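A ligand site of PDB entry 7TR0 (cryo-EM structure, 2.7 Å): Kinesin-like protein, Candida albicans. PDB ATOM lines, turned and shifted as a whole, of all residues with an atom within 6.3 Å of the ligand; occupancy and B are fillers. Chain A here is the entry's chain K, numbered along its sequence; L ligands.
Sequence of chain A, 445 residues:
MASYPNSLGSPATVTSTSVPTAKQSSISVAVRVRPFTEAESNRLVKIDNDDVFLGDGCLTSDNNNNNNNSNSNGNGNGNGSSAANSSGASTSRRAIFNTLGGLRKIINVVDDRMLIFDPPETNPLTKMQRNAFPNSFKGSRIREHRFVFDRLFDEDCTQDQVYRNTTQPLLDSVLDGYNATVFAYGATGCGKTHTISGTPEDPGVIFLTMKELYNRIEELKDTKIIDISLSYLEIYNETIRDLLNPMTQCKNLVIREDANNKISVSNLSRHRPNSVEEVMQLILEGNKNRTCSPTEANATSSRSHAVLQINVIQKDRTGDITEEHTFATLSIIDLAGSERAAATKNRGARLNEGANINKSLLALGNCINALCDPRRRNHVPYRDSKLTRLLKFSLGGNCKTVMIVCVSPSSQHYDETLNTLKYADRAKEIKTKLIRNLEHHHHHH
The backbone NH (N) of Thr 193 lies within hydrogen-bond range of an oxygen (O4) of the ligand, 2.5 Å away.
The side-chain hydroxyl (OG1) of Thr 193 is in hydrogen-bond range of an oxygen (O4) of the ligand, 3.1 Å away.
SG of Cys 190 sits at hydrogen-bond distance from O3 of the ligand (2.8 Å).
O4 of the ligand sits at hydrogen-bond distance from N of Lys 192, at 2.8 Å.
O of Ala 187 lies close to O3 of the ligand.
The backbone NH of Thr 188 sits close to an oxygen (O2) of the ligand, at 3.5 Å.
The backbone NH of Gly 191 lies within hydrogen-bond range of an oxygen (O8) of the ligand, 3.5 Å away.
A ring nitrogen (NE2) of His 194 lies within hydrogen-bond range of a nitrogen (N5) of the ligand (3.3 Å).
N of Lys 192 sits at hydrogen-bond distance from SG of Cys 190, at 3.3 Å.
SG of Cys 190 sits close to O of Cys 406.
The backbone carbonyl oxygen of Gly 189 is in hydrogen-bond range of the guanidinium group of Arg 34 (2.9 Å).
NH2 of Arg 32 lies within hydrogen-bond range of NE2 of His 194.
The side-chain hydroxyl (OG1) of Thr 195 sits at hydrogen-bond distance from the guanidinium group (NH1) of Arg 32 (2.8 Å).
OG1 of Thr 195 lies within hydrogen-bond range of O of Gly 191, 3.3 Å away.
The backbone NH (N) of Glu 40 sits close to the side-chain hydroxyl (OG1) of Thr 37, at 3.2 Å.
OE1 of Glu 40 is in salt-bridge range of NH2 of Arg 34, 2.9 Å away.
A nitrogen (N4) of the ligand sits close to the guanidinium group (NE) of Arg 32 (3.0 Å).
A nitrogen (N1) of the ligand sits close to the backbone NH (N) of Gly 189, at 3.0 Å.
Arg 34 touches the ligand.
Pro 35 touches the ligand (CD to N5, 3.3 Å).
Thr 37 touches the ligand.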
ATOM      1  N   ARG A  32      -5.527 -11.310  11.020  1.00  0.00           N
ATOM      2  CA  ARG A  32      -4.332 -10.878  10.259  1.00  0.00           C
ATOM      3  C   ARG A  32      -3.479  -9.941  11.099  1.00  0.00           C
ATOM      4  O   ARG A  32      -4.034  -8.950  11.610  1.00  0.00           O
ATOM      5  CB  ARG A  32      -4.743 -10.145   8.979  1.00  0.00           C
ATOM      6  CG  ARG A  32      -3.568  -9.636   8.163  1.00  0.00           C
ATOM      7  CD  ARG A  32      -4.000  -9.006   6.853  1.00  0.00           C
ATOM      8  NE  ARG A  32      -2.866  -8.560   6.059  1.00  0.00           N
ATOM      9  CZ  ARG A  32      -2.953  -8.012   4.846  1.00  0.00           C
ATOM     10  NH1 ARG A  32      -4.135  -7.839   4.292  1.00  0.00           N
ATOM     11  NH2 ARG A  32      -1.862  -7.643   4.210  1.00  0.00           N
ATOM     12  N   VAL A  33      -2.184 -10.231  11.211  1.00  0.00           N
ATOM     13  CA  VAL A  33      -1.234  -9.400  11.942  1.00  0.00           C
ATOM     14  C   VAL A  33      -0.504  -8.534  10.928  1.00  0.00           C
ATOM     15  O   VAL A  33       0.074  -9.044   9.963  1.00  0.00           O
ATOM     16  CB  VAL A  33      -0.231 -10.252  12.745  1.00  0.00           C
ATOM     17  CG1 VAL A  33       0.561  -9.375  13.703  1.00  0.00           C
ATOM     18  CG2 VAL A  33      -0.953 -11.363  13.493  1.00  0.00           C
ATOM     19  N   ARG A  34      -0.554  -7.214  11.143  1.00  0.00           N
ATOM     20  CA  ARG A  34       0.111  -6.258  10.225  1.00  0.00           C
ATOM     21  C   ARG A  34       1.575  -6.131  10.607  1.00  0.00           C
ATOM     22  O   ARG A  34       1.917  -6.412  11.770  1.00  0.00           O
ATOM     23  CB  ARG A  34      -0.565  -4.889  10.289  1.00  0.00           C
ATOM     24  CG  ARG A  34      -0.242  -4.082  11.539  1.00  0.00           C
ATOM     25  CD  ARG A  34      -0.947  -2.751  11.504  1.00  0.00           C
ATOM     26  NE  ARG A  34      -0.678  -1.927  12.676  1.00  0.00           N
ATOM     27  CZ  ARG A  34       0.264  -1.000  12.750  1.00  0.00           C
ATOM     28  NH1 ARG A  34       1.049  -0.773  11.707  1.00  0.00           N
ATOM     29  NH2 ARG A  34       0.431  -0.303  13.851  1.00  0.00           N
ATOM     30  N   PRO A  35       2.480  -5.722   9.683  1.00  0.00           N
ATOM     31  CA  PRO A  35       3.878  -5.500  10.024  1.00  0.00           C
ATOM     32  C   PRO A  35       4.116  -4.062  10.516  1.00  0.00           C
ATOM     33  O   PRO A  35       3.479  -3.170  10.011  1.00  0.00           O
ATOM     34  CB  PRO A  35       4.557  -5.713   8.674  1.00  0.00           C
ATOM     35  CG  PRO A  35       3.553  -5.157   7.683  1.00  0.00           C
ATOM     36  CD  PRO A  35       2.205  -5.489   8.267  1.00  0.00           C
ATOM     37  N   THR A  37       5.068  -0.409  10.834  1.00  0.00           N
ATOM     38  CA  THR A  37       5.384   0.608   9.807  1.00  0.00           C
ATOM     39  C   THR A  37       6.795   1.108  10.112  1.00  0.00           C
ATOM     40  O   THR A  37       7.155   1.132  11.300  1.00  0.00           O
ATOM     41  CB  THR A  37       4.374   1.752   9.844  1.00  0.00           C
ATOM     42  OG1 THR A  37       4.518   2.418  11.097  1.00  0.00           O
ATOM     43  CG2 THR A  37       2.947   1.280   9.683  1.00  0.00           C
ATOM     44  N   GLU A  40       6.919   3.448  12.977  1.00  0.00           N
ATOM     45  CA  GLU A  40       6.807   2.782  14.273  1.00  0.00           C
ATOM     46  C   GLU A  40       7.980   1.844  14.519  1.00  0.00           C
ATOM     47  O   GLU A  40       8.423   1.681  15.667  1.00  0.00           O
ATOM     48  CB  GLU A  40       5.479   2.012  14.354  1.00  0.00           C
ATOM     49  CG  GLU A  40       4.229   2.869  14.194  1.00  0.00           C
ATOM     50  CD  GLU A  40       2.971   2.052  13.950  1.00  0.00           C
ATOM     51  OE1 GLU A  40       3.085   0.826  13.736  1.00  0.00           O
ATOM     52  OE2 GLU A  40       1.872   2.638  13.976  1.00  0.00           O
ATOM     53  N   GLU A 155       2.889 -11.477   9.573  1.00  0.00           N
ATOM     54  CA  GLU A 155       3.288 -10.208   8.962  1.00  0.00           C
ATOM     55  C   GLU A 155       3.781 -10.407   7.528  1.00  0.00           C
ATOM     56  O   GLU A 155       3.585  -9.529   6.679  1.00  0.00           O
ATOM     57  CB  GLU A 155       4.371  -9.543   9.808  1.00  0.00           C
ATOM     58  CG  GLU A 155       4.032  -9.420  11.279  1.00  0.00           C
ATOM     59  CD  GLU A 155       5.014  -8.549  12.037  1.00  0.00           C
ATOM     60  OE1 GLU A 155       6.007  -8.085  11.424  1.00  0.00           O
ATOM     61  OE2 GLU A 155       4.799  -8.329  13.252  1.00  0.00           O
ATOM     62  N   CYS A 157       2.866 -12.645   5.214  1.00  0.00           N
ATOM     63  CA  CYS A 157       1.853 -13.002   4.218  1.00  0.00           C
ATOM     64  C   CYS A 157       1.313 -11.746   3.546  1.00  0.00           C
ATOM     65  O   CYS A 157       1.002 -10.747   4.214  1.00  0.00           O
ATOM     66  CB  CYS A 157       0.707 -13.777   4.873  1.00  0.00           C
ATOM     67  SG  CYS A 157       1.197 -15.368   5.579  1.00  0.00           S
ATOM     68  N   TYR A 185     -13.407  -6.411  10.651  1.00  0.00           N
ATOM     69  CA  TYR A 185     -13.423  -5.787  11.973  1.00  0.00           C
ATOM     70  C   TYR A 185     -12.005  -5.408  12.381  1.00  0.00           C
ATOM     71  O   TYR A 185     -11.020  -6.026  11.960  1.00  0.00           O
ATOM     72  CB  TYR A 185     -14.039  -6.713  13.030  1.00  0.00           C
ATOM     73  CG  TYR A 185     -14.255  -6.041  14.376  1.00  0.00           C
ATOM     74  CD1 TYR A 185     -15.050  -4.905  14.490  1.00  0.00           C
ATOM     75  CD2 TYR A 185     -13.665  -6.538  15.522  1.00  0.00           C
ATOM     76  CE1 TYR A 185     -15.238  -4.292  15.707  1.00  0.00           C
ATOM     77  CE2 TYR A 185     -13.846  -5.936  16.746  1.00  0.00           C
ATOM     78  CZ  TYR A 185     -14.633  -4.814  16.831  1.00  0.00           C
ATOM     79  OH  TYR A 185     -14.821  -4.201  18.048  1.00  0.00           O
ATOM     80  N   GLY A 186     -11.916  -4.369  13.197  1.00  0.00           N
ATOM     81  CA  GLY A 186     -10.665  -3.939  13.776  1.00  0.00           C
ATOM     82  C   GLY A 186     -10.793  -2.572  14.398  1.00  0.00           C
ATOM     83  O   GLY A 186     -11.770  -1.844  14.208  1.00  0.00           O
ATOM     84  N   ALA A 187      -9.752  -2.168  15.132  1.00  0.00           N
ATOM     85  CA  ALA A 187      -9.743  -0.813  15.715  1.00  0.00           C
ATOM     86  C   ALA A 187      -8.934   0.104  14.783  1.00  0.00           C
ATOM     87  O   ALA A 187      -8.543  -0.365  13.704  1.00  0.00           O
ATOM     88  CB  ALA A 187      -9.150  -0.846  17.091  1.00  0.00           C
ATOM     89  N   THR A 188      -8.701   1.341  15.200  1.00  0.00           N
ATOM     90  CA  THR A 188      -7.951   2.306  14.353  1.00  0.00           C
ATOM     91  C   THR A 188      -6.483   1.872  14.282  1.00  0.00           C
ATOM     92  O   THR A 188      -5.935   1.492  15.338  1.00  0.00           O
ATOM     93  CB  THR A 188      -8.086   3.734  14.884  1.00  0.00           C
ATOM     94  OG1 THR A 188      -7.685   3.724  16.256  1.00  0.00           O
ATOM     95  CG2 THR A 188      -9.505   4.261  14.771  1.00  0.00           C
ATOM     96  N   GLY A 189      -5.884   1.922  13.094  1.00  0.00           N
ATOM     97  CA  GLY A 189      -4.445   1.575  12.948  1.00  0.00           C
ATOM     98  C   GLY A 189      -4.224   0.087  12.862  1.00  0.00           C
ATOM     99  O   GLY A 189      -3.051  -0.331  12.792  1.00  0.00           O
ATOM    100  N   CYS A 190      -5.292  -0.704  12.869  1.00  0.00           N
ATOM    101  CA  CYS A 190      -5.161  -2.184  12.842  1.00  0.00           C
ATOM    102  C   CYS A 190      -4.741  -2.633  11.446  1.00  0.00           C
ATOM    103  O   CYS A 190      -4.075  -3.681  11.346  1.00  0.00           O
ATOM    104  CB  CYS A 190      -6.490  -2.839  13.209  1.00  0.00           C
ATOM    105  SG  CYS A 190      -7.771  -2.635  11.948  1.00  0.00           S
ATOM    106  N   GLY A 191      -5.107  -1.867  10.414  1.00  0.00           N
ATOM    107  CA  GLY A 191      -4.736  -2.218   9.024  1.00  0.00           C
ATOM    108  C   GLY A 191      -5.915  -2.735   8.217  1.00  0.00           C
ATOM    109  O   GLY A 191      -5.683  -3.297   7.132  1.00  0.00           O
ATOM    110  N   LYS A 192      -7.137  -2.555   8.723  1.00  0.00           N
ATOM    111  CA  LYS A 192      -8.345  -3.073   8.044  1.00  0.00           C
ATOM    112  C   LYS A 192      -8.449  -2.443   6.654  1.00  0.00           C
ATOM    113  O   LYS A 192      -8.735  -3.179   5.700  1.00  0.00           O
ATOM    114  CB  LYS A 192      -9.598  -2.761   8.861  1.00  0.00           C
ATOM    115  CG  LYS A 192     -10.896  -3.364   8.322  1.00  0.00           C
ATOM    116  CD  LYS A 192     -12.065  -3.142   9.240  1.00  0.00           C
ATOM    117  CE  LYS A 192     -12.256  -1.693   9.627  1.00  0.00           C
ATOM    118  NZ  LYS A 192     -13.465  -1.496  10.461  1.00  0.00           N
ATOM    119  N   THR A 193      -8.214  -1.134   6.552  1.00  0.00           N
ATOM    120  CA  THR A 193      -8.372  -0.435   5.258  1.00  0.00           C
ATOM    121  C   THR A 193      -7.432  -1.068   4.226  1.00  0.00           C
ATOM    122  O   THR A 193      -7.901  -1.393   3.122  1.00  0.00           O
ATOM    123  CB  THR A 193      -8.102   1.062   5.414  1.00  0.00           C
ATOM    124  OG1 THR A 193      -8.977   1.553   6.434  1.00  0.00           O
ATOM    125  CG2 THR A 193      -8.313   1.840   4.129  1.00  0.00           C
ATOM    126  N   HIS A 194      -6.165  -1.233   4.591  1.00  0.00           N
ATOM    127  CA  HIS A 194      -5.167  -1.803   3.636  1.00  0.00           C
ATOM    128  C   HIS A 194      -5.681  -3.147   3.142  1.00  0.00           C
ATOM    129  O   HIS A 194      -5.538  -3.428   1.938  1.00  0.00           O
ATOM    130  CB  HIS A 194      -3.793  -1.926   4.302  1.00  0.00           C
ATOM    131  CG  HIS A 194      -2.907  -2.923   3.653  1.00  0.00           C
ATOM    132  ND1 HIS A 194      -2.109  -2.612   2.564  1.00  0.00           N
ATOM    133  CD2 HIS A 194      -2.673  -4.229   3.923  1.00  0.00           C
ATOM    134  CE1 HIS A 194      -1.434  -3.683   2.191  1.00  0.00           C
ATOM    135  NE2 HIS A 194      -1.752  -4.683   3.014  1.00  0.00           N
ATOM    136  N   THR A 195      -6.270  -3.944   4.031  1.00  0.00           N
ATOM    137  CA  THR A 195      -6.732  -5.269   3.655  1.00  0.00           C
ATOM    138  C   THR A 195      -7.935  -5.191   2.710  1.00  0.00           C
ATOM    139  O   THR A 195      -7.884  -5.704   1.588  1.00  0.00           O
ATOM    140  CB  THR A 195      -7.089  -6.082   4.908  1.00  0.00           C
ATOM    141  OG1 THR A 195      -5.915  -6.277   5.697  1.00  0.00           O
ATOM    142  CG2 THR A 195      -7.672  -7.435   4.528  1.00  0.00           C
ATOM    143  N   ASN A 298      -8.350   8.596  14.894  1.00  0.00           N
ATOM    144  CA  ASN A 298      -8.263   8.802  13.452  1.00  0.00           C
ATOM    145  C   ASN A 298      -9.196   9.935  13.050  1.00  0.00           C
ATOM    146  O   ASN A 298     -10.318  10.043  13.566  1.00  0.00           O
ATOM    147  CB  ASN A 298      -8.617   7.528  12.684  1.00  0.00           C
ATOM    148  CG  ASN A 298      -8.563   7.721  11.184  1.00  0.00           C
ATOM    149  OD1 ASN A 298      -9.589   7.892  10.530  1.00  0.00           O
ATOM    150  ND2 ASN A 298      -7.359   7.678  10.625  1.00  0.00           N
ATOM    151  N   CYS A 406      -8.566  -7.606  11.712  1.00  0.00           N
ATOM    152  CA  CYS A 406      -7.218  -7.057  11.591  1.00  0.00           C
ATOM    153  C   CYS A 406      -6.781  -6.449  12.912  1.00  0.00           C
ATOM    154  O   CYS A 406      -7.487  -5.606  13.471  1.00  0.00           O
ATOM    155  CB  CYS A 406      -7.169  -6.018  10.473  1.00  0.00           C
ATOM    156  SG  CYS A 406      -7.645  -6.666   8.859  1.00  0.00           S
HETATM  157  P1  LIG L   1      -8.836   1.078  10.653  1.00  0.00           P
HETATM  158  O1  LIG L   1      -9.630   1.490   9.443  1.00  0.00           O
HETATM  159  O2  LIG L   1      -9.405   1.795  11.842  1.00  0.00           O
HETATM  160  O3  LIG L   1      -9.016  -0.408  10.856  1.00  0.00           O
HETATM  161  P2  LIG L   1      -6.574   1.460   8.954  1.00  0.00           P
HETATM  162  O4  LIG L   1      -6.885   0.195   8.214  1.00  0.00           O
HETATM  163  O5  LIG L   1      -6.798   2.776   8.256  1.00  0.00           O
HETATM  164  N1  LIG L   1      -7.256   1.445  10.435  1.00  0.00           N
HETATM  165  P3  LIG L   1      -3.860   1.338   8.009  1.00  0.00           P
HETATM  166  O6  LIG L   1      -4.110   0.151   7.135  1.00  0.00           O
HETATM  167  O7  LIG L   1      -3.803   2.686   7.365  1.00  0.00           O
HETATM  168  O8  LIG L   1      -4.991   1.378   9.139  1.00  0.00           O
HETATM  169  O9  LIG L   1      -2.533   1.103   8.875  1.00  0.00           O
HETATM  170  C1  LIG L   1      -1.468   2.090   8.813  1.00  0.00           C
HETATM  171  C2  LIG L   1      -0.517   1.739   7.694  1.00  0.00           C
HETATM  172  O10 LIG L   1       0.240   0.551   8.046  1.00  0.00           O
HETATM  173  C3  LIG L   1      -1.147   1.404   6.331  1.00  0.00           C
HETATM  174  O11 LIG L   1      -1.472   2.565   5.594  1.00  0.00           O
HETATM  175  C4  LIG L   1      -0.016   0.590   5.693  1.00  0.00           C
HETATM  176  O12 LIG L   1       1.028   1.400   5.219  1.00  0.00           O
HETATM  177  C5  LIG L   1       0.441  -0.239   6.887  1.00  0.00           C
HETATM  178  N2  LIG L   1      -0.294  -1.486   7.073  1.00  0.00           N
HETATM  179  C6  LIG L   1      -1.414  -1.694   7.828  1.00  0.00           C
HETATM  180  N3  LIG L   1      -1.832  -2.937   7.777  1.00  0.00           N
HETATM  181  C7  LIG L   1      -0.928  -3.574   6.931  1.00  0.00           C
HETATM  182  C8  LIG L   1      -0.831  -4.898   6.477  1.00  0.00           C
HETATM  183  N4  LIG L   1      -1.688  -5.868   6.817  1.00  0.00           N
HETATM  184  N5  LIG L   1       0.190  -5.193   5.643  1.00  0.00           N
HETATM  185  C9  LIG L   1       1.040  -4.213   5.296  1.00  0.00           C
HETATM  186  N6  LIG L   1       1.046  -2.942   5.672  1.00  0.00           N
HETATM  187  C10 LIG L   1       0.018  -2.688   6.496  1.00  0.00           C
